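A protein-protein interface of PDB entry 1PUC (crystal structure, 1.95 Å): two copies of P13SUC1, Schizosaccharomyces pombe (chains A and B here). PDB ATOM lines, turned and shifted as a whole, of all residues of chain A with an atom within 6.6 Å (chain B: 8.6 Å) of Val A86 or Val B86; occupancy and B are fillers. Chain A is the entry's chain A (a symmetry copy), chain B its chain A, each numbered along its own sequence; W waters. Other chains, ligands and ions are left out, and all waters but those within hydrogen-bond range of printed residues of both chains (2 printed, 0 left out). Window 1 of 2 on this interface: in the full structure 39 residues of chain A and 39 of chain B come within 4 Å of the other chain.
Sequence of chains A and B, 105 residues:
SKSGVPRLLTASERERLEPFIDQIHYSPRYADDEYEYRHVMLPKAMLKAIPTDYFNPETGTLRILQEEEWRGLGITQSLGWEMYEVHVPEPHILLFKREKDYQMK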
ATOM      1  N   TYR A  84      27.365  16.905  19.418  1.00  0.00           N
ATOM      2  CA  TYR A  84      25.999  17.187  18.996  1.00  0.00           C
ATOM      3  C   TYR A  84      25.741  16.513  17.664  1.00  0.00           C
ATOM      4  O   TYR A  84      26.663  16.046  17.003  1.00  0.00           O
ATOM      5  CB  TYR A  84      25.727  18.697  18.921  1.00  0.00           C
ATOM      6  CG  TYR A  84      26.276  19.414  17.705  1.00  0.00           C
ATOM      7  CD1 TYR A  84      27.578  19.919  17.692  1.00  0.00           C
ATOM      8  CD2 TYR A  84      25.482  19.612  16.578  1.00  0.00           C
ATOM      9  CE1 TYR A  84      28.066  20.602  16.588  1.00  0.00           C
ATOM     10  CE2 TYR A  84      25.964  20.295  15.466  1.00  0.00           C
ATOM     11  CZ  TYR A  84      27.256  20.789  15.475  1.00  0.00           C
ATOM     12  OH  TYR A  84      27.738  21.461  14.366  1.00  0.00           O
ATOM     13  N   GLU A  85      24.476  16.423  17.294  1.00  0.00           N
ATOM     14  CA  GLU A  85      24.113  15.788  16.046  1.00  0.00           C
ATOM     15  C   GLU A  85      23.120  16.623  15.248  1.00  0.00           C
ATOM     16  O   GLU A  85      22.401  17.470  15.790  1.00  0.00           O
ATOM     17  CB  GLU A  85      23.551  14.388  16.307  1.00  0.00           C
ATOM     18  CG  GLU A  85      22.264  14.357  17.119  1.00  0.00           C
ATOM     19  CD  GLU A  85      21.820  12.942  17.486  1.00  0.00           C
ATOM     20  OE1 GLU A  85      22.345  11.957  16.917  1.00  0.00           O
ATOM     21  OE2 GLU A  85      20.940  12.815  18.363  1.00  0.00           O
ATOM     22  N   VAL A  86      23.138  16.416  13.941  1.00  0.00           N
ATOM     23  CA  VAL A  86      22.246  17.113  13.038  1.00  0.00           C
ATOM     24  C   VAL A  86      20.933  16.337  13.089  1.00  0.00           C
ATOM     25  O   VAL A  86      20.931  15.112  13.183  1.00  0.00           O
ATOM     26  CB  VAL A  86      22.805  17.094  11.603  1.00  0.00           C
ATOM     27  CG1 VAL A  86      21.912  17.875  10.686  1.00  0.00           C
ATOM     28  CG2 VAL A  86      24.205  17.674  11.574  1.00  0.00           C
ATOM     29  N   HIS A  87      19.812  17.041  13.065  1.00  0.00           N
ATOM     30  CA  HIS A  87      18.540  16.353  13.111  1.00  0.00           C
ATOM     31  C   HIS A  87      17.804  16.390  11.770  1.00  0.00           C
ATOM     32  O   HIS A  87      17.398  17.451  11.294  1.00  0.00           O
ATOM     33  CB  HIS A  87      17.688  16.906  14.250  1.00  0.00           C
ATOM     34  CG  HIS A  87      18.281  16.670  15.606  1.00  0.00           C
ATOM     35  ND1 HIS A  87      18.515  15.406  16.106  1.00  0.00           N
ATOM     36  CD2 HIS A  87      18.681  17.533  16.571  1.00  0.00           C
ATOM     37  CE1 HIS A  87      19.033  15.499  17.317  1.00  0.00           C
ATOM     38  NE2 HIS A  87      19.145  16.780  17.624  1.00  0.00           N
ATOM     39  N   VAL A  88      17.717  15.226  11.135  1.00  0.00           N
ATOM     40  CA  VAL A  88      17.038  15.081   9.857  1.00  0.00           C
ATOM     41  C   VAL A  88      15.545  14.850  10.054  1.00  0.00           C
ATOM     42  O   VAL A  88      15.135  14.045  10.891  1.00  0.00           O
ATOM     43  CB  VAL A  88      17.649  13.923   9.048  1.00  0.00           C
ATOM     44  CG1 VAL A  88      16.679  13.422   7.982  1.00  0.00           C
ATOM     45  CG2 VAL A  88      18.917  14.405   8.385  1.00  0.00           C
ATOM     46  N   PRO A  89      14.711  15.566   9.284  1.00  0.00           N
ATOM     47  CA  PRO A  89      13.265  15.398   9.414  1.00  0.00           C
ATOM     48  C   PRO A  89      12.781  14.035   8.914  1.00  0.00           C
ATOM     49  O   PRO A  89      13.385  13.435   8.021  1.00  0.00           O
ATOM     50  CB  PRO A  89      12.724  16.544   8.559  1.00  0.00           C
ATOM     51  CG  PRO A  89      13.756  16.669   7.482  1.00  0.00           C
ATOM     52  CD  PRO A  89      15.035  16.585   8.269  1.00  0.00           C
ATOM     53  N   LEU A  95      11.280  20.196   3.444  1.00  0.00           N
ATOM     54  CA  LEU A  95      11.790  21.525   3.734  1.00  0.00           C
ATOM     55  C   LEU A  95      11.925  22.351   2.465  1.00  0.00           C
ATOM     56  O   LEU A  95      12.373  21.845   1.433  1.00  0.00           O
ATOM     57  CB  LEU A  95      13.150  21.401   4.423  1.00  0.00           C
ATOM     58  CG  LEU A  95      13.250  20.442   5.610  1.00  0.00           C
ATOM     59  CD1 LEU A  95      14.711  20.399   6.070  1.00  0.00           C
ATOM     60  CD2 LEU A  95      12.324  20.858   6.759  1.00  0.00           C
ATOM     61  N   THR B  59      18.574   7.284   1.939  1.00  0.00           N
ATOM     62  CA  THR B  59      18.134   8.102   3.058  1.00  0.00           C
ATOM     63  C   THR B  59      16.767   7.723   3.609  1.00  0.00           C
ATOM     64  O   THR B  59      16.454   8.016   4.766  1.00  0.00           O
ATOM     65  CB  THR B  59      18.104   9.569   2.651  1.00  0.00           C
ATOM     66  OG1 THR B  59      17.267   9.720   1.500  1.00  0.00           O
ATOM     67  CG2 THR B  59      19.498  10.042   2.301  1.00  0.00           C
ATOM     68  N   THR B  61      14.166   9.039   2.736  1.00  0.00           N
ATOM     69  CA  THR B  61      13.354  10.228   2.540  1.00  0.00           C
ATOM     70  C   THR B  61      13.120  10.446   1.045  1.00  0.00           C
ATOM     71  O   THR B  61      13.634   9.699   0.211  1.00  0.00           O
ATOM     72  CB  THR B  61      14.067  11.482   3.107  1.00  0.00           C
ATOM     73  OG1 THR B  61      15.310  11.672   2.423  1.00  0.00           O
ATOM     74  CG2 THR B  61      14.327  11.338   4.612  1.00  0.00           C
ATOM     75  N   ILE B  64      15.390  15.155  -3.587  1.00  0.00           N
ATOM     76  CA  ILE B  64      15.128  16.563  -3.855  1.00  0.00           C
ATOM     77  C   ILE B  64      14.301  16.640  -5.118  1.00  0.00           C
ATOM     78  O   ILE B  64      14.747  16.228  -6.189  1.00  0.00           O
ATOM     79  CB  ILE B  64      16.420  17.380  -4.045  1.00  0.00           C
ATOM     80  CG1 ILE B  64      17.262  17.322  -2.770  1.00  0.00           C
ATOM     81  CG2 ILE B  64      16.081  18.834  -4.361  1.00  0.00           C
ATOM     82  CD1 ILE B  64      16.587  17.952  -1.567  1.00  0.00           C
ATOM     83  N   MET B  83      12.916  23.036  -2.775  1.00  0.00           N
ATOM     84  CA  MET B  83      13.060  21.982  -1.791  1.00  0.00           C
ATOM     85  C   MET B  83      14.531  21.821  -1.452  1.00  0.00           C
ATOM     86  O   MET B  83      15.393  21.948  -2.326  1.00  0.00           O
ATOM     87  CB  MET B  83      12.537  20.669  -2.350  1.00  0.00           C
ATOM     88  CG  MET B  83      12.378  19.591  -1.309  1.00  0.00           C
ATOM     89  SD  MET B  83      11.685  18.130  -2.026  1.00  0.00           S
ATOM     90  CE  MET B  83      12.080  16.939  -0.760  1.00  0.00           C
ATOM     91  N   TYR B  84      14.817  21.549  -0.187  1.00  0.00           N
ATOM     92  CA  TYR B  84      16.193  21.342   0.247  1.00  0.00           C
ATOM     93  C   TYR B  84      16.224  20.263   1.309  1.00  0.00           C
ATOM     94  O   TYR B  84      15.189  19.868   1.838  1.00  0.00           O
ATOM     95  CB  TYR B  84      16.831  22.645   0.754  1.00  0.00           C
ATOM     96  CG  TYR B  84      16.432  23.084   2.147  1.00  0.00           C
ATOM     97  CD1 TYR B  84      15.298  23.871   2.359  1.00  0.00           C
ATOM     98  CD2 TYR B  84      17.206  22.735   3.252  1.00  0.00           C
ATOM     99  CE1 TYR B  84      14.954  24.297   3.634  1.00  0.00           C
ATOM    100  CE2 TYR B  84      16.868  23.157   4.533  1.00  0.00           C
ATOM    101  CZ  TYR B  84      15.741  23.938   4.720  1.00  0.00           C
ATOM    102  OH  TYR B  84      15.401  24.351   5.996  1.00  0.00           O
ATOM    103  N   GLU B  85      17.411  19.755   1.588  1.00  0.00           N
ATOM    104  CA  GLU B  85      17.555  18.710   2.577  1.00  0.00           C
ATOM    105  C   GLU B  85      18.694  18.996   3.548  1.00  0.00           C
ATOM    106  O   GLU B  85      19.622  19.757   3.253  1.00  0.00           O
ATOM    107  CB  GLU B  85      17.759  17.355   1.893  1.00  0.00           C
ATOM    108  CG  GLU B  85      19.028  17.245   1.060  1.00  0.00           C
ATOM    109  CD  GLU B  85      19.118  15.938   0.274  1.00  0.00           C
ATOM    110  OE1 GLU B  85      18.342  14.993   0.546  1.00  0.00           O
ATOM    111  OE2 GLU B  85      19.972  15.860  -0.635  1.00  0.00           O
ATOM    112  N   VAL B  86      18.574  18.423   4.735  1.00  0.00           N
ATOM    113  CA  VAL B  86      19.577  18.577   5.768  1.00  0.00           C
ATOM    114  C   VAL B  86      20.656  17.549   5.440  1.00  0.00           C
ATOM    115  O   VAL B  86      20.355  16.446   4.989  1.00  0.00           O
ATOM    116  CB  VAL B  86      18.976  18.275   7.154  1.00  0.00           C
ATOM    117  CG1 VAL B  86      20.000  18.501   8.226  1.00  0.00           C
ATOM    118  CG2 VAL B  86      17.766  19.151   7.407  1.00  0.00           C
ATOM    119  N   HIS B  87      21.915  17.910   5.628  1.00  0.00           N
ATOM    120  CA  HIS B  87      22.976  16.972   5.333  1.00  0.00           C
ATOM    121  C   HIS B  87      23.645  16.426   6.595  1.00  0.00           C
ATOM    122  O   HIS B  87      24.285  17.162   7.347  1.00  0.00           O
ATOM    123  CB  HIS B  87      23.982  17.605   4.375  1.00  0.00           C
ATOM    124  CG  HIS B  87      23.401  17.936   3.034  1.00  0.00           C
ATOM    125  ND1 HIS B  87      22.878  16.977   2.193  1.00  0.00           N
ATOM    126  CD2 HIS B  87      23.267  19.117   2.383  1.00  0.00           C
ATOM    127  CE1 HIS B  87      22.447  17.550   1.083  1.00  0.00           C
ATOM    128  NE2 HIS B  87      22.670  18.849   1.173  1.00  0.00           N
ATOM    129  N   VAL B  88      23.415  15.143   6.854  1.00  0.00           N
ATOM    130  CA  VAL B  88      23.986  14.462   8.005  1.00  0.00           C
ATOM    131  C   VAL B  88      25.380  13.934   7.692  1.00  0.00           C
ATOM    132  O   VAL B  88      25.608  13.337   6.639  1.00  0.00           O
ATOM    133  CB  VAL B  88      23.074  13.308   8.459  1.00  0.00           C
ATOM    134  CG1 VAL B  88      23.847  12.289   9.292  1.00  0.00           C
ATOM    135  CG2 VAL B  88      21.943  13.874   9.282  1.00  0.00           C
ATOM    136  N   PRO B  89      26.337  14.159   8.605  1.00  0.00           N
ATOM    137  CA  PRO B  89      27.698  13.681   8.376  1.00  0.00           C
ATOM    138  C   PRO B  89      27.807  12.156   8.432  1.00  0.00           C
ATOM    139  O   PRO B  89      27.039  11.489   9.131  1.00  0.00           O
ATOM    140  CB  PRO B  89      28.476  14.350   9.511  1.00  0.00           C
ATOM    141  CG  PRO B  89      27.467  14.405  10.615  1.00  0.00           C
ATOM    142  CD  PRO B  89      26.239  14.880   9.888  1.00  0.00           C
ATOM    143  N   GLU B  90      28.737  11.611   7.652  1.00  0.00           N
ATOM    144  CA  GLU B  90      28.995  10.173   7.619  1.00  0.00           C
ATOM    145  C   GLU B  90      29.361   9.754   9.044  1.00  0.00           C
ATOM    146  O   GLU B  90      29.904  10.555   9.794  1.00  0.00           O
ATOM    147  CB  GLU B  90      30.148   9.880   6.659  1.00  0.00           C
ATOM    148  CG  GLU B  90      29.829  10.203   5.212  1.00  0.00           C
ATOM    149  CD  GLU B  90      31.006   9.967   4.292  1.00  0.00           C
ATOM    150  OE1 GLU B  90      31.287   8.792   3.962  1.00  0.00           O
ATOM    151  OE2 GLU B  90      31.659  10.959   3.901  1.00  0.00           O
ATOM    152  N   ILE B  93      32.478  11.030  11.105  1.00  0.00           N
ATOM    153  CA  ILE B  93      32.643  12.451  11.395  1.00  0.00           C
ATOM    154  C   ILE B  93      31.781  12.817  12.590  1.00  0.00           C
ATOM    155  O   ILE B  93      30.577  12.565  12.608  1.00  0.00           O
ATOM    156  CB  ILE B  93      32.253  13.331  10.185  1.00  0.00           C
ATOM    157  CG1 ILE B  93      33.092  12.938   8.969  1.00  0.00           C
ATOM    158  CG2 ILE B  93      32.482  14.808  10.521  1.00  0.00           C
ATOM    159  CD1 ILE B  93      32.702  13.633   7.693  1.00  0.00           C
ATOM    160  N   LEU B  94      32.411  13.387  13.612  1.00  0.00           N
ATOM    161  CA  LEU B  94      31.716  13.787  14.828  1.00  0.00           C
ATOM    162  C   LEU B  94      31.710  15.312  14.952  1.00  0.00           C
ATOM    163  O   LEU B  94      32.715  15.984  14.675  1.00  0.00           O
ATOM    164  CB  LEU B  94      32.402  13.169  16.051  1.00  0.00           C
ATOM    165  CG  LEU B  94      32.778  11.681  16.031  1.00  0.00           C
ATOM    166  CD1 LEU B  94      33.217  11.252  17.416  1.00  0.00           C
ATOM    167  CD2 LEU B  94      31.597  10.851  15.576  1.00  0.00           C
ATOM    168  N   LEU B  95      30.589  15.847  15.417  1.00  0.00           N
ATOM    169  CA  LEU B  95      30.439  17.285  15.552  1.00  0.00           C
ATOM    170  C   LEU B  95      30.465  17.705  17.013  1.00  0.00           C
ATOM    171  O   LEU B  95      29.866  17.047  17.865  1.00  0.00           O
ATOM    172  CB  LEU B  95      29.118  17.714  14.910  1.00  0.00           C
ATOM    173  CG  LEU B  95      28.827  17.205  13.497  1.00  0.00           C
ATOM    174  CD1 LEU B  95      27.421  17.667  13.102  1.00  0.00           C
ATOM    175  CD2 LEU B  95      29.871  17.697  12.488  1.00  0.00           C
HETATM  176  O   HOH W   1      13.116  18.166   2.398  1.00  0.00           O
HETATM  177  O   HOH W   2      28.265  14.124  15.886  1.00  0.00           O
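The backbone NH (N) of Tyr B84 is in hydrogen-bond range of the backbone carbonyl oxygen (O) of Leu A95, 2.9 Å away.
The backbone NH (N) of Tyr A84 is in hydrogen-bond range of the backbone carbonyl oxygen (O) of Leu B95, at 2.9 Å.
Val B86 touches Val A86.
CD of Pro B89 touches CG2 of Val A86 (3.8 Å).
Val A86 touches Leu B95.
CG2 of Val B88 touches CG2 of Val A88 (3.2 Å).
CD of Pro A89 touches CG2 of Val B86 (3.8 Å).
Leu A95 touches Met B83.
Leu A95 touches Val B86.
Val A86 touches three residues of chain B.
Of the printed residues of chain B, Val A88 touches Val B88 (3.2 Å).
Printed residues of chain A within 4 Å of Val B88: Val A88.
Printed residues of chain A within 4 Å of Leu B95: Tyr A84 (2.9 Å) and Val A86 (3.6 Å).
Of the printed residues of chain B, Leu A95 touches Met B83, Tyr B84 and Val B86.
Glu B85 touches none of the printed residues of chain A.
His A87 touches none of the printed residues of chain B.
The nearest residue of chain B that does not touch Val A86 is Val B88 (4.1 Å).
The nearest printed residue of chain A that does not touch Val B88 is Val A86 (4.1 Å).
Of the 7 printed residues of chain A, 5 touch a printed residue of chain B.
Hydrophobic or aromatic side chains of chain A that line the printed part of chain B: Tyr A84, Val A86, Val A88, Pro A89 and Leu A95.
Hydrophobic or aromatic side chains of chain B that line the printed part of chain A: Met B83, Tyr B84, Val B86, Val B88, Pro B89 and Leu B95.
Tyr A84 touches Leu B95, and with the chains exchanged Leu A95 touches Tyr B84.
Val A86 touches Pro B89, and with the chains exchanged Pro A89 touches Val B86.
Val A86 touches Leu B95, and with the chains exchanged Leu A95 touches Val B86.
Val B88 touches its own counterpart, Val A88.
7 positions are printed for both chains.
Of the 9 pairs that touch across the chains among the printed residues, 8 have their exchanged pair printed and touching as well.
Water W2 bridges the backbone carbonyl oxygen of Tyr A84 and the backbone NH of Leu B95.
Water W1 lies within hydrogen-bond range of O of Tyr B84 and N of Leu A95.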
